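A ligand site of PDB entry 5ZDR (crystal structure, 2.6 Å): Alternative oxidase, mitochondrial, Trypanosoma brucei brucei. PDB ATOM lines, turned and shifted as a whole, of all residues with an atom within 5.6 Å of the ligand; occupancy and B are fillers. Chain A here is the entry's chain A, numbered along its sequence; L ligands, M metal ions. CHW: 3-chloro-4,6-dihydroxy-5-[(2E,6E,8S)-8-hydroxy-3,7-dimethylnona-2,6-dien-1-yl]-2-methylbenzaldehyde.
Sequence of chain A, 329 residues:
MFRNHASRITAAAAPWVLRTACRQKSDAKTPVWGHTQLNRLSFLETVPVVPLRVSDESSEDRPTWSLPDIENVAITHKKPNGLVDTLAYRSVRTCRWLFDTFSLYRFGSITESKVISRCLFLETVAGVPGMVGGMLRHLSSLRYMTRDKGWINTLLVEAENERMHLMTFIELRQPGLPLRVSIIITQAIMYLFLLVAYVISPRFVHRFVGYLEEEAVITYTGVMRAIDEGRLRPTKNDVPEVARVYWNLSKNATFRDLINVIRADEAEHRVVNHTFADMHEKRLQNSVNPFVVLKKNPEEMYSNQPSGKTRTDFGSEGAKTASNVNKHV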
ATOM      1  N   VAL A  92     -20.942  26.412  17.968  1.00  0.00           N
ATOM      2  CA  VAL A  92     -21.398  25.354  18.822  1.00  0.00           C
ATOM      3  C   VAL A  92     -22.423  24.483  18.145  1.00  0.00           C
ATOM      4  O   VAL A  92     -22.461  23.315  18.375  1.00  0.00           O
ATOM      5  CB  VAL A  92     -21.826  25.843  20.228  1.00  0.00           C
ATOM      6  CG1 VAL A  92     -22.508  24.754  21.003  1.00  0.00           C
ATOM      7  CG2 VAL A  92     -20.623  26.306  20.996  1.00  0.00           C
ATOM      8  N   CYS A  95     -20.529  22.399  15.476  1.00  0.00           N
ATOM      9  CA  CYS A  95     -19.944  21.249  16.152  1.00  0.00           C
ATOM     10  C   CYS A  95     -20.910  20.221  16.701  1.00  0.00           C
ATOM     11  O   CYS A  95     -20.615  19.088  16.689  1.00  0.00           O
ATOM     12  CB  CYS A  95     -19.053  21.657  17.299  1.00  0.00           C
ATOM     13  SG  CYS A  95     -17.830  22.859  17.041  1.00  0.00           S
ATOM     14  N   ARG A  96     -22.033  20.616  17.224  1.00  0.00           N
ATOM     15  CA  ARG A  96     -22.957  19.646  17.729  1.00  0.00           C
ATOM     16  C   ARG A  96     -23.391  18.766  16.599  1.00  0.00           C
ATOM     17  O   ARG A  96     -23.528  17.594  16.757  1.00  0.00           O
ATOM     18  CB  ARG A  96     -24.182  20.319  18.356  1.00  0.00           C
ATOM     19  CG  ARG A  96     -24.646  19.685  19.656  1.00  0.00           C
ATOM     20  CD  ARG A  96     -25.855  18.814  19.532  1.00  0.00           C
ATOM     21  NE  ARG A  96     -25.860  17.642  20.392  1.00  0.00           N
ATOM     22  CZ  ARG A  96     -26.430  17.572  21.576  1.00  0.00           C
ATOM     23  NH1 ARG A  96     -27.031  18.581  22.087  1.00  0.00           N
ATOM     24  NH2 ARG A  96     -26.388  16.486  22.268  1.00  0.00           N
ATOM     25  N   PHE A  99     -20.577  16.493  15.237  1.00  0.00           N
ATOM     26  CA  PHE A  99     -20.264  15.489  16.198  1.00  0.00           C
ATOM     27  C   PHE A  99     -21.345  14.461  16.252  1.00  0.00           C
ATOM     28  O   PHE A  99     -21.081  13.317  16.427  1.00  0.00           O
ATOM     29  CB  PHE A  99     -20.031  16.072  17.576  1.00  0.00           C
ATOM     30  CG  PHE A  99     -19.689  15.033  18.596  1.00  0.00           C
ATOM     31  CD1 PHE A  99     -18.393  14.671  18.817  1.00  0.00           C
ATOM     32  CD2 PHE A  99     -20.662  14.382  19.294  1.00  0.00           C
ATOM     33  CE1 PHE A  99     -18.081  13.690  19.691  1.00  0.00           C
ATOM     34  CE2 PHE A  99     -20.353  13.404  20.181  1.00  0.00           C
ATOM     35  CZ  PHE A  99     -19.064  13.054  20.376  1.00  0.00           C
ATOM     36  N   ARG A 118     -19.666   8.847  24.597  1.00  0.00           N
ATOM     37  CA  ARG A 118     -19.860  10.238  24.237  1.00  0.00           C
ATOM     38  C   ARG A 118     -19.387  11.177  25.337  1.00  0.00           C
ATOM     39  O   ARG A 118     -18.473  11.981  25.122  1.00  0.00           O
ATOM     40  CB  ARG A 118     -21.323  10.479  23.926  1.00  0.00           C
ATOM     41  CG  ARG A 118     -21.630  11.927  23.628  1.00  0.00           C
ATOM     42  CD  ARG A 118     -23.090  12.107  23.277  1.00  0.00           C
ATOM     43  NE  ARG A 118     -23.347  13.515  23.038  1.00  0.00           N
ATOM     44  CZ  ARG A 118     -23.633  14.062  21.875  1.00  0.00           C
ATOM     45  NH1 ARG A 118     -23.749  13.323  20.798  1.00  0.00           N
ATOM     46  NH2 ARG A 118     -23.840  15.365  21.782  1.00  0.00           N
ATOM     47  N   CYS A 119     -19.985  11.057  26.508  1.00  0.00           N
ATOM     48  CA  CYS A 119     -19.620  11.897  27.657  1.00  0.00           C
ATOM     49  C   CYS A 119     -18.098  11.836  27.950  1.00  0.00           C
ATOM     50  O   CYS A 119     -17.434  12.866  28.093  1.00  0.00           O
ATOM     51  CB  CYS A 119     -20.426  11.483  28.879  1.00  0.00           C
ATOM     52  SG  CYS A 119     -22.194  11.164  28.560  1.00  0.00           S
ATOM     53  N   PHE A 121     -15.548  11.298  25.799  1.00  0.00           N
ATOM     54  CA  PHE A 121     -14.737  12.023  24.810  1.00  0.00           C
ATOM     55  C   PHE A 121     -14.888  13.528  24.932  1.00  0.00           C
ATOM     56  O   PHE A 121     -13.903  14.279  24.830  1.00  0.00           O
ATOM     57  CB  PHE A 121     -15.094  11.645  23.380  1.00  0.00           C
ATOM     58  CG  PHE A 121     -14.614  12.643  22.372  1.00  0.00           C
ATOM     59  CD1 PHE A 121     -15.441  13.642  21.935  1.00  0.00           C
ATOM     60  CD2 PHE A 121     -13.312  12.638  21.929  1.00  0.00           C
ATOM     61  CE1 PHE A 121     -14.984  14.580  21.044  1.00  0.00           C
ATOM     62  CE2 PHE A 121     -12.849  13.564  21.036  1.00  0.00           C
ATOM     63  CZ  PHE A 121     -13.689  14.546  20.605  1.00  0.00           C
ATOM     64  N   LEU A 122     -16.144  13.953  25.053  1.00  0.00           N
ATOM     65  CA  LEU A 122     -16.467  15.349  25.179  1.00  0.00           C
ATOM     66  C   LEU A 122     -15.975  15.917  26.483  1.00  0.00           C
ATOM     67  O   LEU A 122     -15.491  17.044  26.512  1.00  0.00           O
ATOM     68  CB  LEU A 122     -17.976  15.539  25.059  1.00  0.00           C
ATOM     69  CG  LEU A 122     -18.535  15.417  23.635  1.00  0.00           C
ATOM     70  CD1 LEU A 122     -20.021  15.561  23.694  1.00  0.00           C
ATOM     71  CD2 LEU A 122     -17.981  16.469  22.683  1.00  0.00           C
ATOM     72  N   GLU A 123     -16.086  15.179  27.580  1.00  0.00           N
ATOM     73  CA  GLU A 123     -15.569  15.704  28.846  1.00  0.00           C
ATOM     74  C   GLU A 123     -14.069  15.997  28.759  1.00  0.00           C
ATOM     75  O   GLU A 123     -13.610  16.914  29.419  1.00  0.00           O
ATOM     76  CB  GLU A 123     -15.937  14.822  30.042  1.00  0.00           C
ATOM     77  CG  GLU A 123     -17.434  14.884  30.435  1.00  0.00           C
ATOM     78  CD  GLU A 123     -17.942  16.254  30.947  1.00  0.00           C
ATOM     79  OE1 GLU A 123     -19.062  16.295  31.494  1.00  0.00           O
ATOM     80  OE2 GLU A 123     -17.263  17.304  30.806  1.00  0.00           O
ATOM     81  N   VAL A 125     -12.647  17.770  26.670  1.00  0.00           N
ATOM     82  CA  VAL A 125     -12.462  19.089  26.033  1.00  0.00           C
ATOM     83  C   VAL A 125     -13.237  20.155  26.791  1.00  0.00           C
ATOM     84  O   VAL A 125     -13.046  21.332  26.505  1.00  0.00           O
ATOM     85  CB  VAL A 125     -12.930  19.110  24.548  1.00  0.00           C
ATOM     86  CG1 VAL A 125     -12.280  20.253  23.784  1.00  0.00           C
ATOM     87  CG2 VAL A 125     -12.586  17.835  23.845  1.00  0.00           C
ATOM     88  N   ALA A 126     -14.116  19.750  27.708  1.00  0.00           N
ATOM     89  CA  ALA A 126     -14.783  20.665  28.644  1.00  0.00           C
ATOM     90  C   ALA A 126     -13.831  21.135  29.767  1.00  0.00           C
ATOM     91  O   ALA A 126     -14.022  22.201  30.381  1.00  0.00           O
ATOM     92  CB  ALA A 126     -16.002  19.979  29.244  1.00  0.00           C
ATOM     93  N   GLU A 162     -14.911  19.625  35.790  1.00  0.00           N
ATOM     94  CA  GLU A 162     -15.045  18.919  34.501  1.00  0.00           C
ATOM     95  C   GLU A 162     -13.989  17.807  34.345  1.00  0.00           C
ATOM     96  O   GLU A 162     -14.224  16.755  33.721  1.00  0.00           O
ATOM     97  CB  GLU A 162     -14.970  19.898  33.347  1.00  0.00           C
ATOM     98  CG  GLU A 162     -16.053  20.968  33.317  1.00  0.00           C
ATOM     99  CD  GLU A 162     -17.364  20.468  32.758  1.00  0.00           C
ATOM    100  OE1 GLU A 162     -17.914  19.492  33.323  1.00  0.00           O
ATOM    101  OE2 GLU A 162     -17.851  21.063  31.768  1.00  0.00           O
ATOM    102  N   THR A 186      -7.501  16.154  19.648  1.00  0.00           N
ATOM    103  CA  THR A 186      -8.592  17.139  19.939  1.00  0.00           C
ATOM    104  C   THR A 186      -8.033  18.213  20.850  1.00  0.00           C
ATOM    105  O   THR A 186      -8.301  19.393  20.652  1.00  0.00           O
ATOM    106  CB  THR A 186      -9.792  16.535  20.655  1.00  0.00           C
ATOM    107  OG1 THR A 186     -10.568  15.752  19.747  1.00  0.00           O
ATOM    108  CG2 THR A 186     -10.666  17.628  21.201  1.00  0.00           C
ATOM    109  N   MET A 190      -7.913  22.117  20.249  1.00  0.00           N
ATOM    110  CA  MET A 190      -8.817  22.930  21.049  1.00  0.00           C
ATOM    111  C   MET A 190      -8.070  23.792  22.061  1.00  0.00           C
ATOM    112  O   MET A 190      -8.512  24.907  22.410  1.00  0.00           O
ATOM    113  CB  MET A 190      -9.869  22.061  21.723  1.00  0.00           C
ATOM    114  CG  MET A 190     -10.802  21.354  20.735  1.00  0.00           C
ATOM    115  SD  MET A 190     -11.972  22.348  19.769  1.00  0.00           S
ATOM    116  CE  MET A 190     -12.313  23.769  20.826  1.00  0.00           C
ATOM    117  N   LEU A 212     -21.981  25.885  24.582  1.00  0.00           N
ATOM    118  CA  LEU A 212     -21.491  24.555  24.863  1.00  0.00           C
ATOM    119  C   LEU A 212     -22.329  23.881  25.969  1.00  0.00           C
ATOM    120  O   LEU A 212     -22.955  22.843  25.749  1.00  0.00           O
ATOM    121  CB  LEU A 212     -20.037  24.666  25.320  1.00  0.00           C
ATOM    122  CG  LEU A 212     -18.843  24.137  24.530  1.00  0.00           C
ATOM    123  CD1 LEU A 212     -17.992  23.459  25.577  1.00  0.00           C
ATOM    124  CD2 LEU A 212     -19.216  23.134  23.456  1.00  0.00           C
ATOM    125  N   GLU A 213     -22.370  24.488  27.162  1.00  0.00           N
ATOM    126  CA  GLU A 213     -23.179  23.923  28.278  1.00  0.00           C
ATOM    127  C   GLU A 213     -24.713  23.866  28.042  1.00  0.00           C
ATOM    128  O   GLU A 213     -25.410  23.019  28.616  1.00  0.00           O
ATOM    129  CB  GLU A 213     -22.909  24.709  29.575  1.00  0.00           C
ATOM    130  CG  GLU A 213     -21.436  24.808  29.995  1.00  0.00           C
ATOM    131  CD  GLU A 213     -20.875  23.493  30.435  1.00  0.00           C
ATOM    132  OE1 GLU A 213     -21.206  22.519  29.770  1.00  0.00           O
ATOM    133  OE2 GLU A 213     -20.132  23.423  31.439  1.00  0.00           O
ATOM    134  N   GLU A 215     -25.963  22.860  25.372  1.00  0.00           N
ATOM    135  CA  GLU A 215     -26.011  21.528  24.743  1.00  0.00           C
ATOM    136  C   GLU A 215     -25.703  20.400  25.704  1.00  0.00           C
ATOM    137  O   GLU A 215     -26.255  19.316  25.632  1.00  0.00           O
ATOM    138  CB  GLU A 215     -25.033  21.512  23.622  1.00  0.00           C
ATOM    139  CG  GLU A 215     -25.286  22.622  22.621  1.00  0.00           C
ATOM    140  CD  GLU A 215     -26.587  22.441  21.890  1.00  0.00           C
ATOM    141  OE1 GLU A 215     -26.904  21.286  21.555  1.00  0.00           O
ATOM    142  OE2 GLU A 215     -27.297  23.434  21.651  1.00  0.00           O
ATOM    143  N   ALA A 216     -24.800  20.654  26.637  1.00  0.00           N
ATOM    144  CA  ALA A 216     -24.502  19.660  27.681  1.00  0.00           C
ATOM    145  C   ALA A 216     -25.736  19.382  28.534  1.00  0.00           C
ATOM    146  O   ALA A 216     -25.943  18.226  28.953  1.00  0.00           O
ATOM    147  CB  ALA A 216     -23.395  20.187  28.574  1.00  0.00           C
ATOM    148  N   THR A 219     -28.292  17.256  26.300  1.00  0.00           N
ATOM    149  CA  THR A 219     -27.903  15.867  26.206  1.00  0.00           C
ATOM    150  C   THR A 219     -28.165  15.086  27.486  1.00  0.00           C
ATOM    151  O   THR A 219     -28.572  13.934  27.416  1.00  0.00           O
ATOM    152  CB  THR A 219     -26.428  15.701  25.827  1.00  0.00           C
ATOM    153  OG1 THR A 219     -26.138  16.509  24.677  1.00  0.00           O
ATOM    154  CG2 THR A 219     -26.127  14.249  25.512  1.00  0.00           C
ATOM    155  N   TYR A 220     -27.927  15.681  28.654  1.00  0.00           N
ATOM    156  CA  TYR A 220     -28.076  14.910  29.889  1.00  0.00           C
ATOM    157  C   TYR A 220     -29.525  14.758  30.352  1.00  0.00           C
ATOM    158  O   TYR A 220     -29.871  13.683  30.874  1.00  0.00           O
ATOM    159  CB  TYR A 220     -27.211  15.470  31.029  1.00  0.00           C
ATOM    160  CG  TYR A 220     -25.712  15.142  30.987  1.00  0.00           C
ATOM    161  CD1 TYR A 220     -25.249  13.841  30.912  1.00  0.00           C
ATOM    162  CD2 TYR A 220     -24.768  16.167  31.081  1.00  0.00           C
ATOM    163  CE1 TYR A 220     -23.891  13.571  30.908  1.00  0.00           C
ATOM    164  CE2 TYR A 220     -23.423  15.905  31.058  1.00  0.00           C
ATOM    165  CZ  TYR A 220     -22.982  14.609  30.983  1.00  0.00           C
ATOM    166  OH  TYR A 220     -21.605  14.377  30.993  1.00  0.00           O
ATOM    167  N   GLU A 266     -23.557  21.558  35.028  1.00  0.00           N
ATOM    168  CA  GLU A 266     -23.389  22.155  33.690  1.00  0.00           C
ATOM    169  C   GLU A 266     -24.321  23.335  33.554  1.00  0.00           C
ATOM    170  O   GLU A 266     -24.052  24.305  32.836  1.00  0.00           O
ATOM    171  CB  GLU A 266     -23.582  21.136  32.579  1.00  0.00           C
ATOM    172  CG  GLU A 266     -22.872  19.789  32.783  1.00  0.00           C
ATOM    173  CD  GLU A 266     -21.399  19.725  32.384  1.00  0.00           C
ATOM    174  OE1 GLU A 266     -20.789  18.645  32.672  1.00  0.00           O
ATOM    175  OE2 GLU A 266     -20.825  20.668  31.771  1.00  0.00           O
HETATM  176  OAA CHW L   1     -20.959  20.268  24.510  1.00  0.00           O
HETATM  177  CAB CHW L   1     -21.332  19.068  25.056  1.00  0.00           C
HETATM  178  CAC CHW L   1     -22.341  18.306  24.482  1.00  0.00           C
HETATM  179  CAD CHW L   1     -23.010  18.771  23.236  1.00  0.00           C
HETATM  180  CAE CHW L   1     -22.011  18.524  22.136  1.00  0.00           C
HETATM  181  CAF CHW L   1     -21.570  19.516  21.372  1.00  0.00           C
HETATM  182  CAG CHW L   1     -20.565  19.223  20.305  1.00  0.00           C
HETATM  183  CAH CHW L   1     -19.209  19.668  20.790  1.00  0.00           C
HETATM  184  CAI CHW L   1     -18.181  19.134  19.813  1.00  0.00           C
HETATM  185  CAJ CHW L   1     -16.878  19.439  19.893  1.00  0.00           C
HETATM  186  CAK CHW L   1     -15.936  18.859  18.871  1.00  0.00           C
HETATM  187  OAL CHW L   1     -14.629  19.341  19.163  1.00  0.00           O
HETATM  188  OAM CHW L   1     -19.564  20.661  26.188  1.00  0.00           O
HETATM  189  CAN CHW L   1     -19.646  19.569  26.742  1.00  0.00           C
HETATM  190  CAO CHW L   1     -20.676  18.652  26.192  1.00  0.00           C
HETATM  191  CAP CHW L   1     -22.694  17.111  25.018  1.00  0.00           C
HETATM  192  OAQ CHW L   1     -23.663  16.381  24.427  1.00  0.00           O
HETATM  193  CAR CHW L   1     -22.042  20.942  21.510  1.00  0.00           C
HETATM  194  CAS CHW L   1     -16.325  20.351  20.968  1.00  0.00           C
HETATM  195  CAT CHW L   1     -15.940  17.330  18.911  1.00  0.00           C
HETATM  196  CAU CHW L   1     -21.062  17.361  26.782  1.00  0.00           C
HETATM  197  CAV CHW L   1     -22.044  16.639  26.141  1.00  0.00           C
HETATM  198 CLAW CHW L   1     -22.542  15.050  26.787  1.00  0.00          CL
HETATM  199  CAX CHW L   1     -20.430  16.793  28.016  1.00  0.00           C
HETATM  200 FE    FE M   1     -19.329  21.350  30.413  1.00  0.00          FE
HETATM  201 FE    FE M   2     -18.938  18.162  32.317  1.00  0.00          FE
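Residues that only touch the ligand: Leu 122 (3.4 Å), Glu 215 (3.4 Å), Phe 121 (3.6 Å), Cys 95 (3.6 Å), Phe 99 (3.6 Å), Glu 123 (3.8 Å), Val 92 (3.9 Å) and Ala 216 (3.9 Å). Hydrophobic or aromatic side chains within 4 Å of the ligand: Val 92, Phe 99, Phe 121, Leu 122, Leu 212 and Ala 216.
The side-chain hydroxyl (OG1) of Thr 219 is in hydrogen-bond range of the backbone carbonyl oxygen (O) of Glu 215 (3.0 Å). The guanidinium group (NH2) of Arg 96 sits at hydrogen-bond distance from the side-chain hydroxyl (OG1) of Thr 219 (2.4 Å). The side-chain carboxylate of Glu 215 lies within salt-bridge range of the guanidinium group of Arg 96 (2.8 Å). OH of Tyr 220 lies close to OE1 of Glu 123, at 3.2 Å.
OG1 of Thr 219 sits at hydrogen-bond distance from OAQ of the ligand (2.5 Å). OAQ of the ligand lies within hydrogen-bond range of NH2 of Arg 118. O of Leu 212 sits at hydrogen-bond distance from OAA of the ligand (3.5 Å). NH2 of Arg 96 lies within hydrogen-bond range of OAQ of the ligand (3.5 Å).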
